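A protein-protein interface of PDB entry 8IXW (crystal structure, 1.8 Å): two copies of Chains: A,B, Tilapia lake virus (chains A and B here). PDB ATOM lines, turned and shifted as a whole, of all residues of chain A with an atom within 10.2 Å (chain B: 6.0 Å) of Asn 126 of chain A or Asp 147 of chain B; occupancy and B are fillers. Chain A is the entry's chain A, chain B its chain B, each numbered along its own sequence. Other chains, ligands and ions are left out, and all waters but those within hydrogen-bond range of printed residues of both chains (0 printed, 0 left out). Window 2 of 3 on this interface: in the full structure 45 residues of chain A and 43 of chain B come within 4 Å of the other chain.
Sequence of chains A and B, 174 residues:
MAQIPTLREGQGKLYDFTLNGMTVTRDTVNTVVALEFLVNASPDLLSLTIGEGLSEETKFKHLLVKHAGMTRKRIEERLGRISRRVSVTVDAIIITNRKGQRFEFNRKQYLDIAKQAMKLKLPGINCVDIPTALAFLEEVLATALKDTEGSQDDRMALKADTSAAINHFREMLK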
ATOM      1  N   MET A   1      17.419 -29.280   4.430  1.00  0.00           N
ATOM      2  CA  MET A   1      17.672 -28.081   5.278  1.00  0.00           C
ATOM      3  C   MET A   1      19.131 -27.645   5.241  1.00  0.00           C
ATOM      4  O   MET A   1      20.041 -28.454   5.058  1.00  0.00           O
ATOM      5  CB  MET A   1      17.268 -28.357   6.731  1.00  0.00           C
ATOM      6  CG  MET A   1      15.854 -27.931   7.087  1.00  0.00           C
ATOM      7  SD  MET A   1      15.264 -28.689   8.614  1.00  0.00           S
ATOM      8  CE  MET A   1      13.540 -28.969   8.214  1.00  0.00           C
ATOM      9  N   LEU A 120      17.609 -20.273   7.754  1.00  0.00           N
ATOM     10  CA  LEU A 120      17.151 -20.252   6.366  1.00  0.00           C
ATOM     11  C   LEU A 120      15.777 -20.907   6.222  1.00  0.00           C
ATOM     12  O   LEU A 120      15.525 -21.669   5.287  1.00  0.00           O
ATOM     13  CB  LEU A 120      18.170 -20.934   5.448  1.00  0.00           C
ATOM     14  CG  LEU A 120      19.577 -20.338   5.417  1.00  0.00           C
ATOM     15  CD1 LEU A 120      20.492 -21.151   4.501  1.00  0.00           C
ATOM     16  CD2 LEU A 120      19.559 -18.877   4.988  1.00  0.00           C
ATOM     17  N   LYS A 121      14.879 -20.604   7.157  1.00  0.00           N
ATOM     18  CA  LYS A 121      13.537 -21.160   7.172  1.00  0.00           C
ATOM     19  C   LYS A 121      12.559 -20.207   6.497  1.00  0.00           C
ATOM     20  O   LYS A 121      12.620 -18.990   6.704  1.00  0.00           O
ATOM     21  CB  LYS A 121      13.051 -21.416   8.600  1.00  0.00           C
ATOM     22  CG  LYS A 121      13.886 -22.377   9.426  1.00  0.00           C
ATOM     23  CD  LYS A 121      13.270 -22.581  10.818  1.00  0.00           C
ATOM     24  CE  LYS A 121      13.920 -21.692  11.886  1.00  0.00           C
ATOM     25  NZ  LYS A 121      13.879 -22.312  13.248  1.00  0.00           N
ATOM     26  N   LEU A 122      11.639 -20.766   5.709  1.00  0.00           N
ATOM     27  CA  LEU A 122      10.481 -20.023   5.217  1.00  0.00           C
ATOM     28  C   LEU A 122       9.226 -20.600   5.855  1.00  0.00           C
ATOM     29  O   LEU A 122       8.864 -21.749   5.556  1.00  0.00           O
ATOM     30  CB  LEU A 122      10.382 -20.094   3.695  1.00  0.00           C
ATOM     31  CG  LEU A 122      11.391 -19.272   2.891  1.00  0.00           C
ATOM     32  CD1 LEU A 122      11.223 -19.590   1.405  1.00  0.00           C
ATOM     33  CD2 LEU A 122      11.254 -17.789   3.150  1.00  0.00           C
ATOM     34  N   PRO A 123       8.539 -19.868   6.729  1.00  0.00           N
ATOM     35  CA  PRO A 123       7.337 -20.427   7.374  1.00  0.00           C
ATOM     36  C   PRO A 123       6.285 -20.829   6.351  1.00  0.00           C
ATOM     37  O   PRO A 123       5.857 -20.023   5.520  1.00  0.00           O
ATOM     38  CB  PRO A 123       6.840 -19.289   8.275  1.00  0.00           C
ATOM     39  CG  PRO A 123       7.923 -18.278   8.331  1.00  0.00           C
ATOM     40  CD  PRO A 123       8.953 -18.570   7.293  1.00  0.00           C
ATOM     41  N   GLY A 124       5.864 -22.089   6.421  1.00  0.00           N
ATOM     42  CA  GLY A 124       4.803 -22.592   5.576  1.00  0.00           C
ATOM     43  C   GLY A 124       5.203 -22.937   4.160  1.00  0.00           C
ATOM     44  O   GLY A 124       4.329 -23.297   3.362  1.00  0.00           O
ATOM     45  N   ILE A 125       6.484 -22.844   3.819  1.00  0.00           N
ATOM     46  CA  ILE A 125       6.972 -23.149   2.479  1.00  0.00           C
ATOM     47  C   ILE A 125       8.052 -24.216   2.596  1.00  0.00           C
ATOM     48  O   ILE A 125       8.976 -24.089   3.408  1.00  0.00           O
ATOM     49  CB  ILE A 125       7.497 -21.891   1.763  1.00  0.00           C
ATOM     50  CG1 ILE A 125       6.334 -20.931   1.482  1.00  0.00           C
ATOM     51  CG2 ILE A 125       8.213 -22.252   0.463  1.00  0.00           C
ATOM     52  CD1 ILE A 125       6.658 -19.472   1.691  1.00  0.00           C
ATOM     53  N   ASN A 126       7.930 -25.263   1.781  1.00  0.00           N
ATOM     54  CA  ASN A 126       8.834 -26.410   1.828  1.00  0.00           C
ATOM     55  C   ASN A 126      10.098 -26.152   1.001  1.00  0.00           C
ATOM     56  O   ASN A 126      10.377 -26.815   0.002  1.00  0.00           O
ATOM     57  CB  ASN A 126       8.104 -27.654   1.339  1.00  0.00           C
ATOM     58  CG  ASN A 126       8.741 -28.937   1.827  1.00  0.00           C
ATOM     59  OD1 ASN A 126       9.214 -29.017   2.960  1.00  0.00           O
ATOM     60  ND2 ASN A 126       8.763 -29.952   0.968  1.00  0.00           N
ATOM     61  N   CYS A 127      10.880 -25.172   1.447  1.00  0.00           N
ATOM     62  CA  CYS A 127      12.137 -24.875   0.778  1.00  0.00           C
ATOM     63  C   CYS A 127      13.018 -24.024   1.677  1.00  0.00           C
ATOM     64  O   CYS A 127      12.527 -23.246   2.499  1.00  0.00           O
ATOM     65  CB  CYS A 127      11.906 -24.155  -0.557  1.00  0.00           C
ATOM     66  SG  CYS A 127      13.366 -24.064  -1.617  1.00  0.00           S
ATOM     67  N   VAL A 128      14.331 -24.203   1.512  1.00  0.00           N
ATOM     68  CA  VAL A 128      15.292 -23.277   2.094  1.00  0.00           C
ATOM     69  C   VAL A 128      14.965 -21.859   1.627  1.00  0.00           C
ATOM     70  O   VAL A 128      14.486 -21.641   0.508  1.00  0.00           O
ATOM     71  CB  VAL A 128      16.722 -23.681   1.694  1.00  0.00           C
ATOM     72  CG1 VAL A 128      17.730 -22.605   2.077  1.00  0.00           C
ATOM     73  CG2 VAL A 128      17.098 -25.015   2.330  1.00  0.00           C
ATOM     74  N   ASP A 129      15.210 -20.885   2.505  1.00  0.00           N
ATOM     75  CA  ASP A 129      15.106 -19.480   2.140  1.00  0.00           C
ATOM     76  C   ASP A 129      16.258 -19.141   1.201  1.00  0.00           C
ATOM     77  O   ASP A 129      17.312 -18.661   1.648  1.00  0.00           O
ATOM     78  CB  ASP A 129      15.098 -18.604   3.395  1.00  0.00           C
ATOM     79  CG  ASP A 129      14.907 -17.132   3.084  1.00  0.00           C
ATOM     80  OD1 ASP A 129      15.003 -16.727   1.907  1.00  0.00           O
ATOM     81  OD2 ASP A 129      14.712 -16.366   4.056  1.00  0.00           O
ATOM     82  N   ILE A 130      16.066 -19.406  -0.090  1.00  0.00           N
ATOM     83  CA  ILE A 130      17.143 -19.220  -1.060  1.00  0.00           C
ATOM     84  C   ILE A 130      17.619 -17.767  -1.114  1.00  0.00           C
ATOM     85  O   ILE A 130      18.837 -17.542  -1.142  1.00  0.00           O
ATOM     86  CB  ILE A 130      16.715 -19.728  -2.438  1.00  0.00           C
ATOM     87  CG1 ILE A 130      16.083 -21.123  -2.375  1.00  0.00           C
ATOM     88  CG2 ILE A 130      17.918 -19.715  -3.390  1.00  0.00           C
ATOM     89  CD1 ILE A 130      17.049 -22.228  -2.032  1.00  0.00           C
ATOM     90  N   VAL B 140      18.311 -27.617  -4.284  1.00  0.00           N
ATOM     91  CA  VAL B 140      17.236 -27.501  -3.303  1.00  0.00           C
ATOM     92  C   VAL B 140      16.034 -26.785  -3.907  1.00  0.00           C
ATOM     93  O   VAL B 140      14.883 -27.181  -3.686  1.00  0.00           O
ATOM     94  CB  VAL B 140      17.751 -26.788  -2.038  1.00  0.00           C
ATOM     95  CG1 VAL B 140      16.602 -26.209  -1.234  1.00  0.00           C
ATOM     96  CG2 VAL B 140      18.561 -27.759  -1.190  1.00  0.00           C
ATOM     97  N   ALA B 142      15.295 -26.499  -7.208  1.00  0.00           N
ATOM     98  CA  ALA B 142      14.710 -27.325  -8.259  1.00  0.00           C
ATOM     99  C   ALA B 142      13.732 -28.332  -7.669  1.00  0.00           C
ATOM    100  O   ALA B 142      12.668 -28.590  -8.243  1.00  0.00           O
ATOM    101  CB  ALA B 142      15.811 -28.034  -9.046  1.00  0.00           C
ATOM    102  N   THR B 143      14.068 -28.893  -6.508  1.00  0.00           N
ATOM    103  CA  THR B 143      13.164 -29.820  -5.839  1.00  0.00           C
ATOM    104  C   THR B 143      11.877 -29.122  -5.423  1.00  0.00           C
ATOM    105  O   THR B 143      10.774 -29.622  -5.679  1.00  0.00           O
ATOM    106  CB  THR B 143      13.863 -30.431  -4.624  1.00  0.00           C
ATOM    107  OG1 THR B 143      14.861 -31.358  -5.069  1.00  0.00           O
ATOM    108  CG2 THR B 143      12.865 -31.149  -3.732  1.00  0.00           C
ATOM    109  N   ALA B 144      11.998 -27.955  -4.785  1.00  0.00           N
ATOM    110  CA  ALA B 144      10.820 -27.259  -4.285  1.00  0.00           C
ATOM    111  C   ALA B 144       9.908 -26.822  -5.422  1.00  0.00           C
ATOM    112  O   ALA B 144       8.679 -26.843  -5.285  1.00  0.00           O
ATOM    113  CB  ALA B 144      11.240 -26.050  -3.450  1.00  0.00           C
ATOM    114  N   LEU B 145      10.485 -26.414  -6.550  1.00  0.00           N
ATOM    115  CA  LEU B 145       9.686 -25.929  -7.666  1.00  0.00           C
ATOM    116  C   LEU B 145       8.989 -27.055  -8.418  1.00  0.00           C
ATOM    117  O   LEU B 145       8.106 -26.775  -9.236  1.00  0.00           O
ATOM    118  CB  LEU B 145      10.566 -25.123  -8.623  1.00  0.00           C
ATOM    119  CG  LEU B 145      11.000 -23.745  -8.111  1.00  0.00           C
ATOM    120  CD1 LEU B 145      11.737 -22.972  -9.200  1.00  0.00           C
ATOM    121  CD2 LEU B 145       9.820 -22.931  -7.585  1.00  0.00           C
ATOM    122  N   LYS B 146       9.350 -28.311  -8.152  1.00  0.00           N
ATOM    123  CA  LYS B 146       8.734 -29.450  -8.819  1.00  0.00           C
ATOM    124  C   LYS B 146       7.704 -30.180  -7.963  1.00  0.00           C
ATOM    125  O   LYS B 146       6.945 -30.990  -8.505  1.00  0.00           O
ATOM    126  CB  LYS B 146       9.811 -30.452  -9.267  1.00  0.00           C
ATOM    127  CG  LYS B 146      10.691 -29.969 -10.413  1.00  0.00           C
ATOM    128  CD  LYS B 146      11.596 -31.090 -10.923  1.00  0.00           C
ATOM    129  CE  LYS B 146      12.742 -31.360  -9.957  1.00  0.00           C
ATOM    130  NZ  LYS B 146      13.670 -32.417 -10.451  1.00  0.00           N
ATOM    131  N   ASP B 147       7.642 -29.927  -6.653  1.00  0.00           N
ATOM    132  CA  ASP B 147       6.666 -30.615  -5.798  1.00  0.00           C
ATOM    133  C   ASP B 147       5.337 -29.846  -5.802  1.00  0.00           C
ATOM    134  O   ASP B 147       4.914 -29.200  -4.849  1.00  0.00           O
ATOM    135  CB  ASP B 147       7.247 -30.853  -4.401  1.00  0.00           C
ATOM    136  CG  ASP B 147       7.083 -29.686  -3.424  1.00  0.00           C
ATOM    137  OD1 ASP B 147       6.288 -28.758  -3.638  1.00  0.00           O
ATOM    138  OD2 ASP B 147       7.767 -29.718  -2.381  1.00  0.00           O
ATOM    139  N   THR B 148       4.636 -29.982  -6.925  1.00  0.00           N
ATOM    140  CA  THR B 148       3.438 -29.172  -7.151  1.00  0.00           C
ATOM    141  C   THR B 148       2.253 -29.538  -6.211  1.00  0.00           C
ATOM    142  O   THR B 148       1.154 -29.015  -6.450  1.00  0.00           O
ATOM    143  CB  THR B 148       3.022 -29.277  -8.625  1.00  0.00           C
ATOM    144  OG1 THR B 148       1.975 -28.335  -8.899  1.00  0.00           O
ATOM    145  CG2 THR B 148       2.560 -30.692  -8.988  1.00  0.00           C
ATOM    146  N   GLU B 149       2.419 -30.371  -5.178  1.00  0.00           N
ATOM    147  CA  GLU B 149       1.361 -30.537  -4.185  1.00  0.00           C
ATOM    148  C   GLU B 149       1.004 -29.194  -3.557  1.00  0.00           C
ATOM    149  O   GLU B 149      -0.153 -28.757  -3.591  1.00  0.00           O
ATOM    150  CB  GLU B 149       1.796 -31.519  -3.092  1.00  0.00           C
ATOM    151  CG  GLU B 149       2.279 -32.879  -3.567  1.00  0.00           C
ATOM    152  CD  GLU B 149       3.752 -32.877  -3.926  1.00  0.00           C
ATOM    153  OE1 GLU B 149       4.374 -31.794  -3.860  1.00  0.00           O
ATOM    154  OE2 GLU B 149       4.292 -33.951  -4.269  1.00  0.00           O
ATOM    155  N   GLY B 150       2.000 -28.526  -2.979  1.00  0.00           N
ATOM    156  CA  GLY B 150       1.793 -27.284  -2.264  1.00  0.00           C
ATOM    157  C   GLY B 150       1.317 -26.134  -3.125  1.00  0.00           C
ATOM    158  O   GLY B 150       0.805 -26.335  -4.230  1.00  0.00           O
ATOM    159  N   SER B 151       1.506 -24.917  -2.626  1.00  0.00           N
ATOM    160  CA  SER B 151       0.895 -23.731  -3.212  1.00  0.00           C
ATOM    161  C   SER B 151       1.635 -23.299  -4.471  1.00  0.00           C
ATOM    162  O   SER B 151       2.834 -23.008  -4.426  1.00  0.00           O
ATOM    163  CB  SER B 151       0.891 -22.601  -2.181  1.00  0.00           C
ATOM    164  OG  SER B 151       0.534 -21.367  -2.768  1.00  0.00           O
ATOM    165  N   ARG B 155       5.143 -21.077  -4.876  1.00  0.00           N
ATOM    166  CA  ARG B 155       6.255 -21.423  -5.752  1.00  0.00           C
ATOM    167  C   ARG B 155       6.590 -20.277  -6.698  1.00  0.00           C
ATOM    168  O   ARG B 155       7.768 -20.004  -6.956  1.00  0.00           O
ATOM    169  CB  ARG B 155       5.930 -22.695  -6.536  1.00  0.00           C
ATOM    170  CG  ARG B 155       6.205 -23.966  -5.751  1.00  0.00           C
ATOM    171  CD  ARG B 155       6.001 -25.212  -6.604  1.00  0.00           C
ATOM    172  NE  ARG B 155       4.594 -25.564  -6.744  1.00  0.00           N
ATOM    173  CZ  ARG B 155       3.854 -25.310  -7.816  1.00  0.00           C
ATOM    174  NH1 ARG B 155       4.363 -24.724  -8.888  1.00  0.00           N
ATOM    175  NH2 ARG B 155       2.571 -25.659  -7.815  1.00  0.00           N
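Ala 144 of chain B touches Asn 126 of chain A (CB to O, 3.6 Å).
Asn 126 of chain A touches Asp 147 of chain B (ND2 to OD2, 3.5 Å).
CG1 of Val 140 of chain B touches SG of Cys 127 of chain A, at 3.9 Å.
Ala 144 of chain B touches Cys 127 of chain A.
CG2 of Val 128 of chain A touches CG1 of Val 140 of chain B, at 3.8 Å.
Ile 125 of chain A touches none of the printed residues of chain B.
Asn 126 of chain A touches two residues of chain B.
Printed residues of chain B within 4 Å of Cys 127 of chain A: Val 140 and Ala 144.
Printed residues of chain B within 4 Å of Val 128 of chain A: Val 140.
Of the printed residues of chain A, Val 140 of chain B touches Cys 127 and Val 128.
Of chain A, only Asn 126 (3.6 Å) and Cys 127 (3.4 Å) come within 4 Å of Ala 144 of chain B.
No residue of chain A comes within 4 Å of Thr 148 of chain B.
No residue of chain A comes within 4 Å of Gly 150 of chain B.
The nearest residue of chain B that does not touch Asn 126 of chain A is Val 140 of chain B (5.8 Å).
The nearest printed residue of chain B that does not touch Val 128 of chain A is Ala 144 of chain B (6.1 Å).
Printed residues of chain B that touch a printed residue of chain A: Val 140, Ala 144 and Asp 147.
Of the 12 printed residues of chain A, 3 touch a printed residue of chain B.
Hydrophobic or aromatic side chains of chain A that line the printed part of chain B: Val 128.
Among the printed residues, 5 pairs touch across the chains.
No position is printed for both chains.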
